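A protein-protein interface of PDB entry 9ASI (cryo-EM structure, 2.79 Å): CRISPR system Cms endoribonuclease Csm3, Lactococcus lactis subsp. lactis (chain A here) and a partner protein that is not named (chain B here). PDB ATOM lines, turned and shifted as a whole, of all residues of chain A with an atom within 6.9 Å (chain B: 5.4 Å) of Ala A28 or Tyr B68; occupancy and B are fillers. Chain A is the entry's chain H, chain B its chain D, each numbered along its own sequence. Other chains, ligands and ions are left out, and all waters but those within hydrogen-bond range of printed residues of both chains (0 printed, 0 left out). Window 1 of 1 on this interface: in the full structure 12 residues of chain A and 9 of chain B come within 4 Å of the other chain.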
ATOM      1  N   ASP A  22     -16.281 -23.137  23.021  1.00  0.00           N
ATOM      2  CA  ASP A  22     -15.840 -22.603  24.303  1.00  0.00           C
ATOM      3  C   ASP A  22     -15.918 -21.082  24.332  1.00  0.00           C
ATOM      4  O   ASP A  22     -15.720 -20.422  23.310  1.00  0.00           O
ATOM      5  CB  ASP A  22     -14.403 -23.047  24.617  1.00  0.00           C
ATOM      6  CG  ASP A  22     -13.473 -22.902  23.427  1.00  0.00           C
ATOM      7  OD1 ASP A  22     -13.898 -22.339  22.396  1.00  0.00           O
ATOM      8  OD2 ASP A  22     -12.312 -23.355  23.522  1.00  0.00           O
ATOM      9  N   PHE A  23     -16.216 -20.549  25.521  1.00  0.00           N
ATOM     10  CA  PHE A  23     -15.843 -19.197  25.944  1.00  0.00           C
ATOM     11  C   PHE A  23     -16.434 -18.117  25.029  1.00  0.00           C
ATOM     12  O   PHE A  23     -15.729 -17.392  24.324  1.00  0.00           O
ATOM     13  CB  PHE A  23     -14.315 -19.087  26.033  1.00  0.00           C
ATOM     14  CG  PHE A  23     -13.834 -17.887  26.792  1.00  0.00           C
ATOM     15  CD1 PHE A  23     -14.342 -17.594  28.043  1.00  0.00           C
ATOM     16  CD2 PHE A  23     -12.841 -17.078  26.273  1.00  0.00           C
ATOM     17  CE1 PHE A  23     -13.891 -16.499  28.748  1.00  0.00           C
ATOM     18  CE2 PHE A  23     -12.383 -15.985  26.979  1.00  0.00           C
ATOM     19  CZ  PHE A  23     -12.911 -15.692  28.214  1.00  0.00           C
ATOM     20  N   SER A  24     -17.762 -18.030  25.065  1.00  0.00           N
ATOM     21  CA  SER A  24     -18.504 -16.949  24.415  1.00  0.00           C
ATOM     22  C   SER A  24     -18.832 -15.890  25.465  1.00  0.00           C
ATOM     23  O   SER A  24     -19.796 -16.032  26.220  1.00  0.00           O
ATOM     24  CB  SER A  24     -19.769 -17.484  23.753  1.00  0.00           C
ATOM     25  OG  SER A  24     -20.627 -16.424  23.369  1.00  0.00           O
ATOM     26  N   ALA A  25     -18.045 -14.814  25.492  1.00  0.00           N
ATOM     27  CA  ALA A  25     -18.223 -13.762  26.486  1.00  0.00           C
ATOM     28  C   ALA A  25     -19.576 -13.068  26.310  1.00  0.00           C
ATOM     29  O   ALA A  25     -20.305 -13.292  25.340  1.00  0.00           O
ATOM     30  CB  ALA A  25     -17.088 -12.745  26.396  1.00  0.00           C
ATOM     31  N   ILE A  26     -19.908 -12.205  27.273  1.00  0.00           N
ATOM     32  CA  ILE A  26     -21.241 -11.617  27.354  1.00  0.00           C
ATOM     33  C   ILE A  26     -21.299 -10.225  26.736  1.00  0.00           C
ATOM     34  O   ILE A  26     -22.292  -9.515  26.919  1.00  0.00           O
ATOM     35  CB  ILE A  26     -21.751 -11.581  28.803  1.00  0.00           C
ATOM     36  CG1 ILE A  26     -20.833 -10.725  29.673  1.00  0.00           C
ATOM     37  CG2 ILE A  26     -21.870 -12.989  29.356  1.00  0.00           C
ATOM     38  CD1 ILE A  26     -21.357 -10.489  31.069  1.00  0.00           C
ATOM     39  N   GLY A  27     -20.254  -9.802  26.037  1.00  0.00           N
ATOM     40  CA  GLY A  27     -20.346  -8.567  25.287  1.00  0.00           C
ATOM     41  C   GLY A  27     -19.541  -8.558  24.006  1.00  0.00           C
ATOM     42  O   GLY A  27     -19.395  -7.508  23.375  1.00  0.00           O
ATOM     43  N   ALA A  28     -19.007  -9.712  23.611  1.00  0.00           N
ATOM     44  CA  ALA A  28     -18.014  -9.772  22.546  1.00  0.00           C
ATOM     45  C   ALA A  28     -18.496 -10.527  21.314  1.00  0.00           C
ATOM     46  O   ALA A  28     -18.514  -9.964  20.216  1.00  0.00           O
ATOM     47  CB  ALA A  28     -16.731 -10.404  23.092  1.00  0.00           C
ATOM     48  N   VAL A  29     -18.878 -11.792  21.459  1.00  0.00           N
ATOM     49  CA  VAL A  29     -19.375 -12.597  20.346  1.00  0.00           C
ATOM     50  C   VAL A  29     -20.502 -13.478  20.856  1.00  0.00           C
ATOM     51  O   VAL A  29     -20.464 -13.972  21.987  1.00  0.00           O
ATOM     52  CB  VAL A  29     -18.272 -13.458  19.681  1.00  0.00           C
ATOM     53  CG1 VAL A  29     -17.183 -12.598  19.075  1.00  0.00           C
ATOM     54  CG2 VAL A  29     -17.668 -14.426  20.690  1.00  0.00           C
ATOM     55  N   ASP A  30     -21.520 -13.656  20.018  1.00  0.00           N
ATOM     56  CA  ASP A  30     -22.624 -14.547  20.329  1.00  0.00           C
ATOM     57  C   ASP A  30     -22.682 -15.764  19.422  1.00  0.00           C
ATOM     58  O   ASP A  30     -23.286 -16.770  19.807  1.00  0.00           O
ATOM     59  CB  ASP A  30     -23.954 -13.786  20.250  1.00  0.00           C
ATOM     60  CG  ASP A  30     -23.909 -12.468  20.999  1.00  0.00           C
ATOM     61  OD1 ASP A  30     -23.530 -12.473  22.187  1.00  0.00           O
ATOM     62  OD2 ASP A  30     -24.248 -11.426  20.407  1.00  0.00           O
ATOM     63  N   VAL A 117     -16.343  -8.785  12.923  1.00  0.00           N
ATOM     64  CA  VAL A 117     -17.495  -8.852  13.810  1.00  0.00           C
ATOM     65  C   VAL A 117     -18.630  -8.075  13.165  1.00  0.00           C
ATOM     66  O   VAL A 117     -18.462  -6.906  12.801  1.00  0.00           O
ATOM     67  CB  VAL A 117     -17.169  -8.303  15.209  1.00  0.00           C
ATOM     68  CG1 VAL A 117     -18.438  -7.979  15.948  1.00  0.00           C
ATOM     69  CG2 VAL A 117     -16.354  -9.315  15.987  1.00  0.00           C
ATOM     70  N   PHE A 119     -22.503  -6.648  13.545  1.00  0.00           N
ATOM     71  CA  PHE A 119     -23.482  -6.246  14.544  1.00  0.00           C
ATOM     72  C   PHE A 119     -24.860  -6.225  13.896  1.00  0.00           C
ATOM     73  O   PHE A 119     -25.126  -5.408  13.012  1.00  0.00           O
ATOM     74  CB  PHE A 119     -23.128  -4.883  15.125  1.00  0.00           C
ATOM     75  CG  PHE A 119     -21.869  -4.878  15.937  1.00  0.00           C
ATOM     76  CD1 PHE A 119     -20.644  -4.663  15.337  1.00  0.00           C
ATOM     77  CD2 PHE A 119     -21.911  -5.081  17.304  1.00  0.00           C
ATOM     78  CE1 PHE A 119     -19.484  -4.652  16.081  1.00  0.00           C
ATOM     79  CE2 PHE A 119     -20.752  -5.068  18.052  1.00  0.00           C
ATOM     80  CZ  PHE A 119     -19.539  -4.859  17.438  1.00  0.00           C
ATOM     81  N   GLN A 134     -24.106 -10.399  17.812  1.00  0.00           N
ATOM     82  CA  GLN A 134     -22.738 -10.093  17.412  1.00  0.00           C
ATOM     83  C   GLN A 134     -22.181 -11.332  16.719  1.00  0.00           C
ATOM     84  O   GLN A 134     -21.690 -12.248  17.383  1.00  0.00           O
ATOM     85  CB  GLN A 134     -21.913  -9.699  18.628  1.00  0.00           C
ATOM     86  CG  GLN A 134     -20.837  -8.689  18.355  1.00  0.00           C
ATOM     87  CD  GLN A 134     -20.464  -7.907  19.590  1.00  0.00           C
ATOM     88  OE1 GLN A 134     -21.321  -7.562  20.402  1.00  0.00           O
ATOM     89  NE2 GLN A 134     -19.176  -7.625  19.745  1.00  0.00           N
ATOM     90  N   ILE A 135     -22.252 -11.349  15.392  1.00  0.00           N
ATOM     91  CA  ILE A 135     -21.899 -12.523  14.604  1.00  0.00           C
ATOM     92  C   ILE A 135     -20.452 -12.375  14.163  1.00  0.00           C
ATOM     93  O   ILE A 135     -20.107 -11.425  13.452  1.00  0.00           O
ATOM     94  CB  ILE A 135     -22.817 -12.692  13.382  1.00  0.00           C
ATOM     95  CG1 ILE A 135     -24.267 -12.907  13.792  1.00  0.00           C
ATOM     96  CG2 ILE A 135     -22.376 -13.868  12.545  1.00  0.00           C
ATOM     97  CD1 ILE A 135     -25.031 -11.627  13.942  1.00  0.00           C
ATOM     98  N   GLU A 136     -19.600 -13.300  14.585  1.00  0.00           N
ATOM     99  CA  GLU A 136     -18.291 -13.398  13.963  1.00  0.00           C
ATOM    100  C   GLU A 136     -18.455 -13.890  12.534  1.00  0.00           C
ATOM    101  O   GLU A 136     -19.326 -14.711  12.234  1.00  0.00           O
ATOM    102  CB  GLU A 136     -17.381 -14.338  14.745  1.00  0.00           C
ATOM    103  CG  GLU A 136     -15.909 -14.097  14.492  1.00  0.00           C
ATOM    104  CD  GLU A 136     -15.051 -15.252  14.949  1.00  0.00           C
ATOM    105  OE1 GLU A 136     -15.618 -16.256  15.425  1.00  0.00           O
ATOM    106  OE2 GLU A 136     -13.812 -15.157  14.833  1.00  0.00           O
ATOM    107  N   VAL B  64     -13.348  -3.179  26.504  1.00  0.00           N
ATOM    108  CA  VAL B  64     -12.617  -4.423  26.727  1.00  0.00           C
ATOM    109  C   VAL B  64     -12.970  -5.451  25.659  1.00  0.00           C
ATOM    110  O   VAL B  64     -12.125  -6.263  25.266  1.00  0.00           O
ATOM    111  CB  VAL B  64     -12.889  -4.948  28.150  1.00  0.00           C
ATOM    112  CG1 VAL B  64     -12.337  -6.354  28.328  1.00  0.00           C
ATOM    113  CG2 VAL B  64     -12.281  -4.008  29.177  1.00  0.00           C
ATOM    114  N   ASN B  65     -14.206  -5.428  25.157  1.00  0.00           N
ATOM    115  CA  ASN B  65     -14.600  -6.359  24.105  1.00  0.00           C
ATOM    116  C   ASN B  65     -13.946  -6.036  22.768  1.00  0.00           C
ATOM    117  O   ASN B  65     -13.801  -6.935  21.934  1.00  0.00           O
ATOM    118  CB  ASN B  65     -16.118  -6.361  23.936  1.00  0.00           C
ATOM    119  CG  ASN B  65     -16.832  -7.044  25.083  1.00  0.00           C
ATOM    120  OD1 ASN B  65     -16.434  -8.119  25.529  1.00  0.00           O
ATOM    121  ND2 ASN B  65     -17.897  -6.418  25.565  1.00  0.00           N
ATOM    122  N   LYS B  66     -13.566  -4.778  22.539  1.00  0.00           N
ATOM    123  CA  LYS B  66     -12.904  -4.419  21.290  1.00  0.00           C
ATOM    124  C   LYS B  66     -11.564  -5.130  21.157  1.00  0.00           C
ATOM    125  O   LYS B  66     -11.224  -5.638  20.082  1.00  0.00           O
ATOM    126  CB  LYS B  66     -12.703  -2.908  21.217  1.00  0.00           C
ATOM    127  CG  LYS B  66     -13.978  -2.088  21.242  1.00  0.00           C
ATOM    128  CD  LYS B  66     -14.805  -2.256  19.986  1.00  0.00           C
ATOM    129  CE  LYS B  66     -16.067  -1.422  20.069  1.00  0.00           C
ATOM    130  NZ  LYS B  66     -15.747   0.031  20.035  1.00  0.00           N
ATOM    131  N   VAL B  67     -10.789  -5.170  22.238  1.00  0.00           N
ATOM    132  CA  VAL B  67      -9.488  -5.824  22.213  1.00  0.00           C
ATOM    133  C   VAL B  67      -9.593  -7.321  22.476  1.00  0.00           C
ATOM    134  O   VAL B  67      -8.787  -8.097  21.955  1.00  0.00           O
ATOM    135  CB  VAL B  67      -8.540  -5.157  23.221  1.00  0.00           C
ATOM    136  CG1 VAL B  67      -8.068  -3.832  22.689  1.00  0.00           C
ATOM    137  CG2 VAL B  67      -9.244  -4.953  24.546  1.00  0.00           C
ATOM    138  N   TYR B  68     -10.568  -7.750  23.279  1.00  0.00           N
ATOM    139  CA  TYR B  68     -10.692  -9.170  23.579  1.00  0.00           C
ATOM    140  C   TYR B  68     -11.114  -9.959  22.348  1.00  0.00           C
ATOM    141  O   TYR B  68     -10.714 -11.117  22.179  1.00  0.00           O
ATOM    142  CB  TYR B  68     -11.686  -9.378  24.723  1.00  0.00           C
ATOM    143  CG  TYR B  68     -12.292 -10.762  24.763  1.00  0.00           C
ATOM    144  CD1 TYR B  68     -11.644 -11.807  25.401  1.00  0.00           C
ATOM    145  CD2 TYR B  68     -13.514 -11.019  24.163  1.00  0.00           C
ATOM    146  CE1 TYR B  68     -12.196 -13.067  25.433  1.00  0.00           C
ATOM    147  CE2 TYR B  68     -14.070 -12.274  24.190  1.00  0.00           C
ATOM    148  CZ  TYR B  68     -13.411 -13.293  24.825  1.00  0.00           C
ATOM    149  OH  TYR B  68     -13.984 -14.542  24.844  1.00  0.00           O
ATOM    150  N   ASN B  69     -11.925  -9.352  21.479  1.00  0.00           N
ATOM    151  CA  ASN B  69     -12.407 -10.048  20.293  1.00  0.00           C
ATOM    152  C   ASN B  69     -11.286 -10.382  19.320  1.00  0.00           C
ATOM    153  O   ASN B  69     -11.427 -11.320  18.529  1.00  0.00           O
ATOM    154  CB  ASN B  69     -13.474  -9.207  19.595  1.00  0.00           C
ATOM    155  CG  ASN B  69     -14.871  -9.622  19.977  1.00  0.00           C
ATOM    156  OD1 ASN B  69     -15.087 -10.746  20.418  1.00  0.00           O
ATOM    157  ND2 ASN B  69     -15.828  -8.718  19.813  1.00  0.00           N
ATOM    158  N   ARG B  70     -10.183  -9.641  19.362  1.00  0.00           N
ATOM    159  CA  ARG B  70      -9.028  -9.923  18.521  1.00  0.00           C
ATOM    160  C   ARG B  70      -7.956 -10.732  19.232  1.00  0.00           C
ATOM    161  O   ARG B  70      -7.216 -11.471  18.575  1.00  0.00           O
ATOM    162  CB  ARG B  70      -8.421  -8.613  18.010  1.00  0.00           C
ATOM    163  CG  ARG B  70      -9.453  -7.582  17.596  1.00  0.00           C
ATOM    164  CD  ARG B  70      -8.792  -6.329  17.052  1.00  0.00           C
ATOM    165  NE  ARG B  70      -7.623  -5.952  17.835  1.00  0.00           N
ATOM    166  CZ  ARG B  70      -7.528  -4.844  18.557  1.00  0.00           C
ATOM    167  NH1 ARG B  70      -8.521  -3.973  18.620  1.00  0.00           N
ATOM    168  NH2 ARG B  70      -6.409  -4.605  19.232  1.00  0.00           N
ATOM    169  N   VAL B  71      -7.852 -10.609  20.556  1.00  0.00           N
ATOM    170  CA  VAL B  71      -6.885 -11.407  21.302  1.00  0.00           C
ATOM    171  C   VAL B  71      -7.305 -12.871  21.330  1.00  0.00           C
ATOM    172  O   VAL B  71      -6.469 -13.773  21.205  1.00  0.00           O
ATOM    173  CB  VAL B  71      -6.711 -10.841  22.724  1.00  0.00           C
ATOM    174  CG1 VAL B  71      -5.973 -11.832  23.611  1.00  0.00           C
ATOM    175  CG2 VAL B  71      -5.971  -9.519  22.681  1.00  0.00           C
ATOM    176  N   ILE B  72      -8.606 -13.131  21.480  1.00  0.00           N
ATOM    177  CA  ILE B  72      -9.058 -14.491  21.752  1.00  0.00           C
ATOM    178  C   ILE B  72      -8.813 -15.417  20.566  1.00  0.00           C
ATOM    179  O   ILE B  72      -8.588 -16.620  20.751  1.00  0.00           O
ATOM    180  CB  ILE B  72     -10.537 -14.484  22.180  1.00  0.00           C
ATOM    181  CG1 ILE B  72     -10.888 -15.803  22.870  1.00  0.00           C
ATOM    182  CG2 ILE B  72     -11.454 -14.226  20.996  1.00  0.00           C
ATOM    183  CD1 ILE B  72     -10.193 -15.990  24.195  1.00  0.00           C
ATOM    184  N   ASN B  73      -8.834 -14.895  19.342  1.00  0.00           N
ATOM    185  CA  ASN B  73      -8.639 -15.736  18.159  1.00  0.00           C
ATOM    186  C   ASN B  73      -7.158 -15.923  17.841  1.00  0.00           C
ATOM    187  O   ASN B  73      -6.727 -15.767  16.700  1.00  0.00           O
ATOM    188  CB  ASN B  73      -9.375 -15.130  16.971  1.00  0.00           C
ATOM    189  CG  ASN B  73     -10.849 -14.920  17.240  1.00  0.00           C
ATOM    190  OD1 ASN B  73     -11.431 -13.923  16.815  1.00  0.00           O
ATOM    191  ND2 ASN B  73     -11.462 -15.861  17.947  1.00  0.00           N
ATOM    192  N   PHE B 129      -3.993 -10.656  29.979  1.00  0.00           N
ATOM    193  CA  PHE B 129      -5.158  -9.939  29.475  1.00  0.00           C
ATOM    194  C   PHE B 129      -6.394 -10.827  29.444  1.00  0.00           C
ATOM    195  O   PHE B 129      -7.512 -10.327  29.592  1.00  0.00           O
ATOM    196  CB  PHE B 129      -4.903  -9.370  28.081  1.00  0.00           C
ATOM    197  CG  PHE B 129      -6.146  -8.840  27.424  1.00  0.00           C
ATOM    198  CD1 PHE B 129      -6.656  -7.604  27.776  1.00  0.00           C
ATOM    199  CD2 PHE B 129      -6.825  -9.593  26.484  1.00  0.00           C
ATOM    200  CE1 PHE B 129      -7.806  -7.124  27.190  1.00  0.00           C
ATOM    201  CE2 PHE B 129      -7.973  -9.116  25.897  1.00  0.00           C
ATOM    202  CZ  PHE B 129      -8.463  -7.882  26.251  1.00  0.00           C
ATOM    203  N   LEU B 130      -6.225 -12.131  29.232  1.00  0.00           N
ATOM    204  CA  LEU B 130      -7.377 -13.024  29.280  1.00  0.00           C
ATOM    205  C   LEU B 130      -7.999 -13.029  30.671  1.00  0.00           C
ATOM    206  O   LEU B 130      -9.228 -12.980  30.815  1.00  0.00           O
ATOM    207  CB  LEU B 130      -6.965 -14.433  28.857  1.00  0.00           C
ATOM    208  CG  LEU B 130      -6.881 -14.694  27.351  1.00  0.00           C
ATOM    209  CD1 LEU B 130      -6.863 -16.187  27.071  1.00  0.00           C
ATOM    210  CD2 LEU B 130      -8.026 -14.020  26.607  1.00  0.00           C
ATOM    211  N   ALA B 133      -9.832  -9.709  31.132  1.00  0.00           N
ATOM    212  CA  ALA B 133     -11.134  -9.756  30.478  1.00  0.00           C
ATOM    213  C   ALA B 133     -12.124 -10.583  31.286  1.00  0.00           C
ATOM    214  O   ALA B 133     -13.296 -10.212  31.409  1.00  0.00           O
ATOM    215  CB  ALA B 133     -10.991 -10.314  29.063  1.00  0.00           C
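Ile B72 touches Phe A23. Ala A25 touches Tyr B68 (CB to CE2, 3.8 Å). CB of Ala A28 touches OD1 of Asn B65 (3.4 Å). Tyr B68 touches Ala A28. OD1 of Asn B69 touches CG1 of Val A29, at 3.1 Å. Val A117 touches Asn B69. NE2 of Gln A134 touches ND2 of Asn B69, 3.5 Å away.
Printed residues of chain B within 4 Å of Ala A28: Asn B65, Tyr B68 and Asn B69. Printed residues of chain B within 4 Å of Glu A136: Asn B73 (3.3 Å). Of the printed residues of chain B, Gly A27 touches Asn B65. The nearest printed residue of chain B that does not touch Ala A28 is Lys B66 (6.5 Å). The nearest printed residue of chain B that does not touch Ala A25 is Asn B65 (4.8 Å).
The backbone carbonyl oxygen (O) of Gly A27 sits at hydrogen-bond distance from the side-chain amide nitrogen (ND2) of Asn B65 (2.9 Å). O of Phe A23 sits close to OH of Tyr B68. O of Ala A28 is in hydrogen-bond range of ND2 of Asn B69, 3.0 Å away. The side-chain amide oxygen (OD1) of Asn B73 sits close to the side-chain carboxylate (OE2) of Glu A136 (3.3 Å).
Of the 14 printed residues of chain A, 8 touch a printed residue of chain B. Hydrophobic or aromatic side chains of chain A within 4 Å of the printed part of chain B: Phe A23, Ala A25, Ala A28, Val A29 and Val A117. Of the 13 printed residues of chain B, 5 touch a printed residue of chain A. Hydrophobic or aromatic side chains of chain B within 4 Å of the printed part of chain A: Tyr B68 and Ile B72. Among the printed residues, no Asp or Glu carboxylate lies within 4 Å of a Lys or Arg side-chain nitrogen of the other chain.
OD2 of Asp A30 sits at hydrogen-bond distance from N of Gln A134, at 2.8 Å. The backbone carbonyl oxygen (O) of Asn B69 lies close to the side-chain amide oxygen (OD1) of Asn B73. NE2 of Gln A134 is in hydrogen-bond range of O of Ala A28 (2.5 Å). The side-chain amide nitrogen (ND2) of Asn B69 lies close to the backbone carbonyl oxygen (O) of Asn B65, at 3.4 Å. The backbone carbonyl oxygen (O) of Val A29 lies within hydrogen-bond range of the side-chain hydroxyl (OG) of Ser A24 (2.8 Å).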
